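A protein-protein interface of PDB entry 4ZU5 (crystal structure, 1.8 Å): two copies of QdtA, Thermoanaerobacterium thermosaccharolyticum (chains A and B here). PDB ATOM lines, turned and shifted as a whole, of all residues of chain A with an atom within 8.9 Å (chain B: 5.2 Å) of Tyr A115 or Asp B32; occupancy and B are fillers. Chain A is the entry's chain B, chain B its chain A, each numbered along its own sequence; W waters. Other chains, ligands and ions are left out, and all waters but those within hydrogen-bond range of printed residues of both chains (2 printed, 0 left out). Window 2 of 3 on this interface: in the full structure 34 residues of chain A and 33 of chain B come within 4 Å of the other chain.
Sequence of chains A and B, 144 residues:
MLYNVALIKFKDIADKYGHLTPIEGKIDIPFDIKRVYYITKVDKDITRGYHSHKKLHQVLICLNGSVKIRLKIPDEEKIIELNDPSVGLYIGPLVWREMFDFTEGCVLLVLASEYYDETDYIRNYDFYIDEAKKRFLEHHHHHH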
ATOM      1  N   ASP A  32     -19.347   7.589  -0.087  1.00  0.00           N
ATOM      2  CA  ASP A  32     -20.735   7.570   0.366  1.00  0.00           C
ATOM      3  C   ASP A  32     -21.644   7.780  -0.822  1.00  0.00           C
ATOM      4  O   ASP A  32     -21.347   8.623  -1.675  1.00  0.00           O
ATOM      5  CB  ASP A  32     -21.011   8.727   1.330  1.00  0.00           C
ATOM      6  CG  ASP A  32     -20.593   8.440   2.749  1.00  0.00           C
ATOM      7  OD1 ASP A  32     -21.029   7.409   3.295  1.00  0.00           O
ATOM      8  OD2 ASP A  32     -19.903   9.319   3.322  1.00  0.00           O
ATOM      9  N   ILE A  33     -22.808   7.152  -0.790  1.00  0.00           N
ATOM     10  CA  ILE A  33     -23.738   7.155  -1.924  1.00  0.00           C
ATOM     11  C   ILE A  33     -24.678   8.331  -1.636  1.00  0.00           C
ATOM     12  O   ILE A  33     -25.556   8.179  -0.815  1.00  0.00           O
ATOM     13  CB  ILE A  33     -24.553   5.857  -1.972  1.00  0.00           C
ATOM     14  CG1 ILE A  33     -23.645   4.655  -2.212  1.00  0.00           C
ATOM     15  CG2 ILE A  33     -25.616   5.897  -3.071  1.00  0.00           C
ATOM     16  CD1 ILE A  33     -24.313   3.301  -1.974  1.00  0.00           C
ATOM     17  N   LYS A  34     -24.488   9.486  -2.267  1.00  0.00           N
ATOM     18  CA  LYS A  34     -25.377  10.643  -2.090  1.00  0.00           C
ATOM     19  C   LYS A  34     -26.571  10.556  -3.017  1.00  0.00           C
ATOM     20  O   LYS A  34     -27.588  11.167  -2.787  1.00  0.00           O
ATOM     21  CB  LYS A  34     -24.629  11.941  -2.350  1.00  0.00           C
ATOM     22  CG  LYS A  34     -23.464  12.176  -1.386  1.00  0.00           C
ATOM     23  CD  LYS A  34     -23.928  12.993  -0.199  1.00  0.00           C
ATOM     24  CE  LYS A  34     -22.800  13.843   0.389  1.00  0.00           C
ATOM     25  NZ  LYS A  34     -21.785  12.924   0.974  1.00  0.00           N
ATOM     26  N   ARG A  35     -26.368   9.918  -4.165  1.00  0.00           N
ATOM     27  CA  ARG A  35     -27.357   9.887  -5.237  1.00  0.00           C
ATOM     28  C   ARG A  35     -27.254   8.566  -5.961  1.00  0.00           C
ATOM     29  O   ARG A  35     -26.151   8.100  -6.190  1.00  0.00           O
ATOM     30  CB  ARG A  35     -27.041  10.984  -6.257  1.00  0.00           C
ATOM     31  CG  ARG A  35     -27.827  10.817  -7.546  1.00  0.00           C
ATOM     32  CD  ARG A  35     -27.786  12.106  -8.312  1.00  0.00           C
ATOM     33  NE  ARG A  35     -26.398  12.540  -8.407  1.00  0.00           N
ATOM     34  CZ  ARG A  35     -25.815  12.752  -9.577  1.00  0.00           C
ATOM     35  NH1 ARG A  35     -24.558  13.215  -9.632  1.00  0.00           N
ATOM     36  NH2 ARG A  35     -26.563  12.614 -10.667  1.00  0.00           N
ATOM     37  N   VAL A  36     -28.373   8.023  -6.410  1.00  0.00           N
ATOM     38  CA  VAL A  36     -28.352   6.904  -7.375  1.00  0.00           C
ATOM     39  C   VAL A  36     -29.282   7.341  -8.512  1.00  0.00           C
ATOM     40  O   VAL A  36     -30.130   8.246  -8.365  1.00  0.00           O
ATOM     41  CB  VAL A  36     -28.831   5.536  -6.814  1.00  0.00           C
ATOM     42  CG1 VAL A  36     -28.147   5.147  -5.504  1.00  0.00           C
ATOM     43  CG2 VAL A  36     -30.320   5.496  -6.596  1.00  0.00           C
ATOM     44  N   HIS A  53     -16.989  14.515 -15.862  1.00  0.00           N
ATOM     45  CA  HIS A  53     -17.136  15.377 -14.672  1.00  0.00           C
ATOM     46  C   HIS A  53     -15.788  15.684 -14.131  1.00  0.00           C
ATOM     47  O   HIS A  53     -14.933  14.819 -14.260  1.00  0.00           O
ATOM     48  CB  HIS A  53     -17.792  14.609 -13.546  1.00  0.00           C
ATOM     49  CG  HIS A  53     -19.075  13.965 -13.920  1.00  0.00           C
ATOM     50  ND1 HIS A  53     -20.292  14.575 -13.707  1.00  0.00           N
ATOM     51  CD2 HIS A  53     -19.338  12.738 -14.426  1.00  0.00           C
ATOM     52  CE1 HIS A  53     -21.250  13.778 -14.144  1.00  0.00           C
ATOM     53  NE2 HIS A  53     -20.699  12.652 -14.566  1.00  0.00           N
ATOM     54  N   LYS A  55     -15.299  16.401 -10.653  1.00  0.00           N
ATOM     55  CA  LYS A  55     -15.203  16.110  -9.252  1.00  0.00           C
ATOM     56  C   LYS A  55     -15.937  14.821  -8.824  1.00  0.00           C
ATOM     57  O   LYS A  55     -15.721  14.317  -7.752  1.00  0.00           O
ATOM     58  CB  LYS A  55     -15.771  17.319  -8.495  1.00  0.00           C
ATOM     59  CG  LYS A  55     -14.935  18.575  -8.671  1.00  0.00           C
ATOM     60  CD  LYS A  55     -15.346  19.690  -7.692  1.00  0.00           C
ATOM     61  CE  LYS A  55     -16.757  20.225  -7.966  1.00  0.00           C
ATOM     62  NZ  LYS A  55     -17.288  21.113  -6.880  1.00  0.00           N
ATOM     63  N   LEU A  56     -16.826  14.305  -9.643  1.00  0.00           N
ATOM     64  CA  LEU A  56     -17.706  13.213  -9.232  1.00  0.00           C
ATOM     65  C   LEU A  56     -17.023  11.851  -9.385  1.00  0.00           C
ATOM     66  O   LEU A  56     -16.269  11.612 -10.362  1.00  0.00           O
ATOM     67  CB  LEU A  56     -18.948  13.270 -10.111  1.00  0.00           C
ATOM     68  CG  LEU A  56     -20.019  12.251  -9.822  1.00  0.00           C
ATOM     69  CD1 LEU A  56     -20.637  12.665  -8.485  1.00  0.00           C
ATOM     70  CD2 LEU A  56     -21.048  12.334 -10.930  1.00  0.00           C
ATOM     71  N   HIS A  57     -17.312  10.964  -8.425  1.00  0.00           N
ATOM     72  CA  HIS A  57     -16.957   9.565  -8.534  1.00  0.00           C
ATOM     73  C   HIS A  57     -18.247   8.766  -8.646  1.00  0.00           C
ATOM     74  O   HIS A  57     -19.282   9.099  -8.022  1.00  0.00           O
ATOM     75  CB  HIS A  57     -16.095   9.120  -7.351  1.00  0.00           C
ATOM     76  CG  HIS A  57     -14.836   9.899  -7.224  1.00  0.00           C
ATOM     77  ND1 HIS A  57     -13.608   9.396  -7.589  1.00  0.00           N
ATOM     78  CD2 HIS A  57     -14.620  11.166  -6.805  1.00  0.00           C
ATOM     79  CE1 HIS A  57     -12.679  10.312  -7.366  1.00  0.00           C
ATOM     80  NE2 HIS A  57     -13.273  11.400  -6.907  1.00  0.00           N
ATOM     81  N   ALA A 112     -23.495   7.481  -7.179  1.00  0.00           N
ATOM     82  CA  ALA A 112     -22.674   8.690  -7.310  1.00  0.00           C
ATOM     83  C   ALA A 112     -22.305   9.329  -5.980  1.00  0.00           C
ATOM     84  O   ALA A 112     -23.114   9.300  -5.016  1.00  0.00           O
ATOM     85  CB  ALA A 112     -23.421   9.706  -8.147  1.00  0.00           C
ATOM     86  N   SER A 113     -21.100   9.911  -5.952  1.00  0.00           N
ATOM     87  CA  SER A 113     -20.512  10.432  -4.729  1.00  0.00           C
ATOM     88  C   SER A 113     -20.939  11.849  -4.383  1.00  0.00           C
ATOM     89  O   SER A 113     -20.541  12.287  -3.332  1.00  0.00           O
ATOM     90  CB  SER A 113     -18.988  10.440  -4.765  1.00  0.00           C
ATOM     91  OG  SER A 113     -18.551  11.417  -5.697  1.00  0.00           O
ATOM     92  N   GLU A 114     -21.761  12.525  -5.191  1.00  0.00           N
ATOM     93  CA  GLU A 114     -22.247  13.842  -4.822  1.00  0.00           C
ATOM     94  C   GLU A 114     -23.627  14.075  -5.370  1.00  0.00           C
ATOM     95  O   GLU A 114     -24.065  13.411  -6.307  1.00  0.00           O
ATOM     96  CB  GLU A 114     -21.359  14.924  -5.429  1.00  0.00           C
ATOM     97  CG  GLU A 114     -19.878  14.893  -5.099  1.00  0.00           C
ATOM     98  CD  GLU A 114     -19.543  15.306  -3.674  1.00  0.00           C
ATOM     99  OE1 GLU A 114     -20.414  15.738  -2.870  1.00  0.00           O
ATOM    100  OE2 GLU A 114     -18.376  15.063  -3.328  1.00  0.00           O
ATOM    101  N   TYR A 115     -24.359  15.036  -4.813  1.00  0.00           N
ATOM    102  CA  TYR A 115     -25.643  15.443  -5.436  1.00  0.00           C
ATOM    103  C   TYR A 115     -25.400  16.078  -6.791  1.00  0.00           C
ATOM    104  O   TYR A 115     -24.311  16.613  -7.052  1.00  0.00           O
ATOM    105  CB  TYR A 115     -26.367  16.463  -4.552  1.00  0.00           C
ATOM    106  CG  TYR A 115     -26.626  15.938  -3.170  1.00  0.00           C
ATOM    107  CD1 TYR A 115     -25.811  16.301  -2.094  1.00  0.00           C
ATOM    108  CD2 TYR A 115     -27.646  15.017  -2.940  1.00  0.00           C
ATOM    109  CE1 TYR A 115     -26.039  15.798  -0.816  1.00  0.00           C
ATOM    110  CE2 TYR A 115     -27.885  14.515  -1.667  1.00  0.00           C
ATOM    111  CZ  TYR A 115     -27.083  14.892  -0.612  1.00  0.00           C
ATOM    112  OH  TYR A 115     -27.306  14.382   0.656  1.00  0.00           O
ATOM    113  N   TYR A 116     -26.401  16.002  -7.657  1.00  0.00           N
ATOM    114  CA  TYR A 116     -26.321  16.569  -8.986  1.00  0.00           C
ATOM    115  C   TYR A 116     -25.920  18.049  -8.923  1.00  0.00           C
ATOM    116  O   TYR A 116     -26.356  18.795  -8.048  1.00  0.00           O
ATOM    117  CB  TYR A 116     -27.608  16.321  -9.766  1.00  0.00           C
ATOM    118  CG  TYR A 116     -27.674  17.098 -11.023  1.00  0.00           C
ATOM    119  CD1 TYR A 116     -27.014  16.671 -12.161  1.00  0.00           C
ATOM    120  CD2 TYR A 116     -28.375  18.286 -11.068  1.00  0.00           C
ATOM    121  CE1 TYR A 116     -27.055  17.406 -13.318  1.00  0.00           C
ATOM    122  CE2 TYR A 116     -28.430  19.035 -12.222  1.00  0.00           C
ATOM    123  CZ  TYR A 116     -27.784  18.575 -13.343  1.00  0.00           C
ATOM    124  OH  TYR A 116     -27.865  19.331 -14.472  1.00  0.00           O
ATOM    125  N   ASP A 117     -24.974  18.411  -9.775  1.00  0.00           N
ATOM    126  CA  ASP A 117     -24.420  19.754  -9.845  1.00  0.00           C
ATOM    127  C   ASP A 117     -24.102  20.010 -11.316  1.00  0.00           C
ATOM    128  O   ASP A 117     -23.100  19.508 -11.827  1.00  0.00           O
ATOM    129  CB  ASP A 117     -23.145  19.809  -8.999  1.00  0.00           C
ATOM    130  CG  ASP A 117     -22.406  21.121  -9.125  1.00  0.00           C
ATOM    131  OD1 ASP A 117     -22.990  22.150  -9.548  1.00  0.00           O
ATOM    132  OD2 ASP A 117     -21.215  21.080  -8.761  1.00  0.00           O
ATOM    133  N   GLU A 118     -24.970  20.747 -12.008  1.00  0.00           N
ATOM    134  CA  GLU A 118     -24.742  20.987 -13.432  1.00  0.00           C
ATOM    135  C   GLU A 118     -23.375  21.600 -13.643  1.00  0.00           C
ATOM    136  O   GLU A 118     -22.678  21.211 -14.574  1.00  0.00           O
ATOM    137  CB  GLU A 118     -25.861  21.774 -14.146  1.00  0.00           C
ATOM    138  CG  GLU A 118     -25.709  21.913 -15.680  1.00  0.00           C
ATOM    139  CD  GLU A 118     -25.589  20.599 -16.462  1.00  0.00           C
ATOM    140  OE1 GLU A 118     -26.108  19.571 -15.974  1.00  0.00           O
ATOM    141  OE2 GLU A 118     -24.961  20.561 -17.563  1.00  0.00           O
ATOM    142  N   THR A 119     -22.920  22.449 -12.734  1.00  0.00           N
ATOM    143  CA  THR A 119     -21.611  23.064 -12.951  1.00  0.00           C
ATOM    144  C   THR A 119     -20.450  22.078 -13.037  1.00  0.00           C
ATOM    145  O   THR A 119     -19.339  22.464 -13.363  1.00  0.00           O
ATOM    146  CB  THR A 119     -21.265  24.164 -11.909  1.00  0.00           C
ATOM    147  OG1 THR A 119     -20.797  23.596 -10.678  1.00  0.00           O
ATOM    148  CG2 THR A 119     -22.451  25.065 -11.650  1.00  0.00           C
ATOM    149  N   ASP A 120     -20.660  20.820 -12.683  1.00  0.00           N
ATOM    150  CA  ASP A 120     -19.578  19.852 -12.738  1.00  0.00           C
ATOM    151  C   ASP A 120     -19.839  18.782 -13.802  1.00  0.00           C
ATOM    152  O   ASP A 120     -19.081  17.801 -13.888  1.00  0.00           O
ATOM    153  CB  ASP A 120     -19.385  19.208 -11.358  1.00  0.00           C
ATOM    154  CG  ASP A 120     -18.271  18.148 -11.347  1.00  0.00           C
ATOM    155  OD1 ASP A 120     -17.140  18.430 -11.824  1.00  0.00           O
ATOM    156  OD2 ASP A 120     -18.573  16.996 -10.954  1.00  0.00           O
ATOM    157  N   TYR A 121     -20.904  18.954 -14.583  1.00  0.00           N
ATOM    158  CA  TYR A 121     -21.219  18.056 -15.712  1.00  0.00           C
ATOM    159  C   TYR A 121     -20.639  18.708 -16.955  1.00  0.00           C
ATOM    160  O   TYR A 121     -21.120  19.759 -17.384  1.00  0.00           O
ATOM    161  CB  TYR A 121     -22.736  17.878 -15.923  1.00  0.00           C
ATOM    162  CG  TYR A 121     -23.304  16.683 -15.192  1.00  0.00           C
ATOM    163  CD1 TYR A 121     -23.082  16.517 -13.805  1.00  0.00           C
ATOM    164  CD2 TYR A 121     -24.029  15.696 -15.860  1.00  0.00           C
ATOM    165  CE1 TYR A 121     -23.573  15.413 -13.103  1.00  0.00           C
ATOM    166  CE2 TYR A 121     -24.542  14.592 -15.167  1.00  0.00           C
ATOM    167  CZ  TYR A 121     -24.313  14.443 -13.789  1.00  0.00           C
ATOM    168  OH  TYR A 121     -24.786  13.341 -13.096  1.00  0.00           O
ATOM    169  N   GLU B  24     -31.960  11.205  -5.065  1.00  0.00           N
ATOM    170  CA  GLU B  24     -30.968  11.830  -4.189  1.00  0.00           C
ATOM    171  C   GLU B  24     -31.400  11.713  -2.715  1.00  0.00           C
ATOM    172  O   GLU B  24     -32.561  11.918  -2.432  1.00  0.00           O
ATOM    173  CB  GLU B  24     -30.797  13.301  -4.531  1.00  0.00           C
ATOM    174  CG  GLU B  24     -30.265  13.526  -5.948  1.00  0.00           C
ATOM    175  CD  GLU B  24     -29.605  14.890  -6.103  1.00  0.00           C
ATOM    176  OE1 GLU B  24     -30.107  15.856  -5.492  1.00  0.00           O
ATOM    177  OE2 GLU B  24     -28.529  14.970  -6.744  1.00  0.00           O
ATOM    178  N   GLY B  25     -30.483  11.295  -1.837  1.00  0.00           N
ATOM    179  CA  GLY B  25     -30.775  11.119  -0.429  1.00  0.00           C
ATOM    180  C   GLY B  25     -31.240  12.412   0.217  1.00  0.00           C
ATOM    181  O   GLY B  25     -30.764  13.499  -0.143  1.00  0.00           O
ATOM    182  N   LYS B  26     -32.319  12.295   0.987  1.00  0.00           N
ATOM    183  CA  LYS B  26     -32.916  13.396   1.712  1.00  0.00           C
ATOM    184  C   LYS B  26     -33.760  14.321   0.844  1.00  0.00           C
ATOM    185  O   LYS B  26     -34.490  15.194   1.370  1.00  0.00           O
ATOM    186  CB  LYS B  26     -31.886  14.181   2.520  1.00  0.00           C
ATOM    187  CG  LYS B  26     -31.218  13.385   3.623  1.00  0.00           C
ATOM    188  CD  LYS B  26     -30.617  14.285   4.703  1.00  0.00           C
ATOM    189  CE  LYS B  26     -29.546  15.198   4.116  1.00  0.00           C
ATOM    190  NZ  LYS B  26     -28.645  15.783   5.142  1.00  0.00           N
ATOM    191  N   ILE B  27     -33.719  14.141  -0.467  1.00  0.00           N
ATOM    192  CA  ILE B  27     -34.501  14.954  -1.406  1.00  0.00           C
ATOM    193  C   ILE B  27     -35.614  14.084  -1.970  1.00  0.00           C
ATOM    194  O   ILE B  27     -36.755  14.258  -1.585  1.00  0.00           O
ATOM    195  CB  ILE B  27     -33.608  15.572  -2.532  1.00  0.00           C
ATOM    196  CG1 ILE B  27     -32.595  16.559  -1.870  1.00  0.00           C
ATOM    197  CG2 ILE B  27     -34.461  16.234  -3.588  1.00  0.00           C
ATOM    198  CD1 ILE B  27     -31.452  17.063  -2.749  1.00  0.00           C
ATOM    199  N   PRO B  30     -36.726  10.438   2.106  1.00  0.00           N
ATOM    200  CA  PRO B  30     -36.510  11.180   3.316  1.00  0.00           C
ATOM    201  C   PRO B  30     -35.233  10.867   4.109  1.00  0.00           C
ATOM    202  O   PRO B  30     -34.948  11.636   5.024  1.00  0.00           O
ATOM    203  CB  PRO B  30     -37.792  10.904   4.127  1.00  0.00           C
ATOM    204  CG  PRO B  30     -38.285   9.584   3.597  1.00  0.00           C
ATOM    205  CD  PRO B  30     -37.970   9.641   2.141  1.00  0.00           C
ATOM    206  N   PHE B  31     -34.373   9.930   3.679  1.00  0.00           N
ATOM    207  CA  PHE B  31     -33.182   9.557   4.456  1.00  0.00           C
ATOM    208  C   PHE B  31     -31.934   9.547   3.582  1.00  0.00           C
ATOM    209  O   PHE B  31     -32.059   9.582   2.377  1.00  0.00           O
ATOM    210  CB  PHE B  31     -33.398   8.186   5.141  1.00  0.00           C
ATOM    211  CG  PHE B  31     -33.794   7.062   4.215  1.00  0.00           C
ATOM    212  CD1 PHE B  31     -32.853   6.325   3.536  1.00  0.00           C
ATOM    213  CD2 PHE B  31     -35.132   6.674   4.095  1.00  0.00           C
ATOM    214  CE1 PHE B  31     -33.223   5.263   2.734  1.00  0.00           C
ATOM    215  CE2 PHE B  31     -35.501   5.625   3.310  1.00  0.00           C
ATOM    216  CZ  PHE B  31     -34.566   4.934   2.593  1.00  0.00           C
ATOM    217  N   ASP B  32     -30.741   9.539   4.167  1.00  0.00           N
ATOM    218  CA  ASP B  32     -29.511   9.346   3.388  1.00  0.00           C
ATOM    219  C   ASP B  32     -29.352   7.875   3.120  1.00  0.00           C
ATOM    220  O   ASP B  32     -29.614   7.029   3.989  1.00  0.00           O
ATOM    221  CB  ASP B  32     -28.252   9.747   4.164  1.00  0.00           C
ATOM    222  CG  ASP B  32     -28.095  11.244   4.291  1.00  0.00           C
ATOM    223  OD1 ASP B  32     -27.921  11.904   3.243  1.00  0.00           O
ATOM    224  OD2 ASP B  32     -28.133  11.715   5.450  1.00  0.00           O
ATOM    225  N   ILE B  33     -28.833   7.571   1.947  1.00  0.00           N
ATOM    226  CA  ILE B  33     -28.598   6.198   1.532  1.00  0.00           C
ATOM    227  C   ILE B  33     -27.236   5.719   2.078  1.00  0.00           C
ATOM    228  O   ILE B  33     -26.164   6.141   1.595  1.00  0.00           O
ATOM    229  CB  ILE B  33     -28.597   6.104  -0.002  1.00  0.00           C
ATOM    230  CG1 ILE B  33     -29.851   6.755  -0.611  1.00  0.00           C
ATOM    231  CG2 ILE B  33     -28.425   4.666  -0.445  1.00  0.00           C
ATOM    232  CD1 ILE B  33     -29.756   7.014  -2.096  1.00  0.00           C
ATOM    233  N   LYS B  34     -27.279   4.839   3.071  1.00  0.00           N
ATOM    234  CA  LYS B  34     -26.049   4.267   3.634  1.00  0.00           C
ATOM    235  C   LYS B  34     -25.731   2.960   2.917  1.00  0.00           C
ATOM    236  O   LYS B  34     -24.590   2.500   2.919  1.00  0.00           O
ATOM    237  CB  LYS B  34     -26.143   4.035   5.149  1.00  0.00           C
ATOM    238  CG  LYS B  34     -26.480   5.287   5.949  1.00  0.00           C
ATOM    239  CD  LYS B  34     -25.233   5.907   6.546  1.00  0.00           C
ATOM    240  CE  LYS B  34     -25.564   6.788   7.756  1.00  0.00           C
ATOM    241  NZ  LYS B  34     -26.271   8.027   7.304  1.00  0.00           N
ATOM    242  N   ALA B 112     -31.495   1.788   1.713  1.00  0.00           N
ATOM    243  CA  ALA B 112     -31.590   1.552   3.138  1.00  0.00           C
ATOM    244  C   ALA B 112     -30.914   2.682   3.866  1.00  0.00           C
ATOM    245  O   ALA B 112     -29.859   3.154   3.432  1.00  0.00           O
ATOM    246  CB  ALA B 112     -30.924   0.235   3.510  1.00  0.00           C
ATOM    247  N   SER B 113     -31.527   3.082   4.974  1.00  0.00           N
ATOM    248  CA  SER B 113     -31.082   4.217   5.801  1.00  0.00           C
ATOM    249  C   SER B 113     -29.908   3.909   6.767  1.00  0.00           C
ATOM    250  O   SER B 113     -29.362   4.838   7.353  1.00  0.00           O
ATOM    251  CB  SER B 113     -32.258   4.777   6.624  1.00  0.00           C
ATOM    252  OG  SER B 113     -32.636   3.932   7.693  1.00  0.00           O
HETATM  253  O   HOH W   1     -23.417   5.515   1.434  1.00  0.00           O
HETATM  254  O   HOH W   2     -27.862   9.680   0.332  1.00  0.00           O
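O of Ala A112 is in hydrogen-bond range of N of Lys A34 (3.1 Å). O of Arg A35 sits at hydrogen-bond distance from N of Ala A112 (2.9 Å). The guanidinium group (NE) of Arg A35 lies within hydrogen-bond range of the backbone carbonyl oxygen (O) of Glu A114 (3.3 Å). OH of Tyr A121 lies within hydrogen-bond range of NH2 of Arg A35 (3.1 Å).
Tyr A115 touches just these residues of chain B: Glu B24, Gly B25 and Asp B32. Asp B32 touches just one residue of chain A: Tyr A115. Gly B25 touches just these residues of chain A: Lys A34 (3.0 Å) and Tyr A115 (3.4 Å). Of the printed residues of chain B, Arg A35 touches Glu B24 (3.3 Å). Of the printed residues of chain B, Lys A34 touches Glu B24 (3.7 Å) and Gly B25 (3.0 Å). Of the printed residues of chain B, Ile A33 touches Ile B33. The nearest residue of chain B that does not touch Tyr A115 is Lys B26 (4.2 Å). The nearest residue of chain A that does not touch Asp B32 is Lys A34 (5.4 Å). The nearest printed residue of chain A that does not touch Glu B24 is Glu A114 (4.7 Å).
OE2 of Glu B24 lies within salt-bridge range of NE of Arg A35 (3.6 Å). The backbone NH (N) of Tyr A116 is in hydrogen-bond range of the side-chain carboxylate (OE2) of Glu B24 (2.5 Å). N of Gly B25 is in hydrogen-bond range of O of Lys A34, 3.0 Å away. O of Ile B33 lies close to O of Ile A33, 3.2 Å away.
Water W1 lies within hydrogen-bond range of O of Ile B33 (2.8 Å) and N of Ile A33 (2.8 Å). Water W2 lies within hydrogen-bond range of the backbone NH (N) of Ile B33 (2.8 Å), the backbone carbonyl oxygen (O) of Ile A33 (3.0 Å) and the backbone carbonyl oxygen (O) of Lys A34 (3.5 Å).
Ile B33 touches its own counterpart, Ile A33. Of the 8 pairs that touch across the chains among the printed residues, 1 has its exchanged pair printed and touching as well.
Hydrophobic or aromatic side chains of chain A that line the printed part of chain B: Ile A33, Tyr A115 and Tyr A116. Of the 11 printed residues of chain B, 4 touch a printed residue of chain A. Hydrophobic or aromatic side chains of chain B that line the printed part of chain A: Ile B33. Among the printed residues, Asp or Glu carboxylates within 4 Å of a Lys or Arg side-chain nitrogen of the other chain: Arg A35 with Glu B24 (3.6 Å).
Among the printed residues, merely in contact across the chains: Tyr A115 with Glu B24 (3.2 Å), Tyr A115 with Gly B25 (3.4 Å), Tyr A115 with Asp B32 (3.6 Å) and Lys A34 with Glu B24 (3.7 Å).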
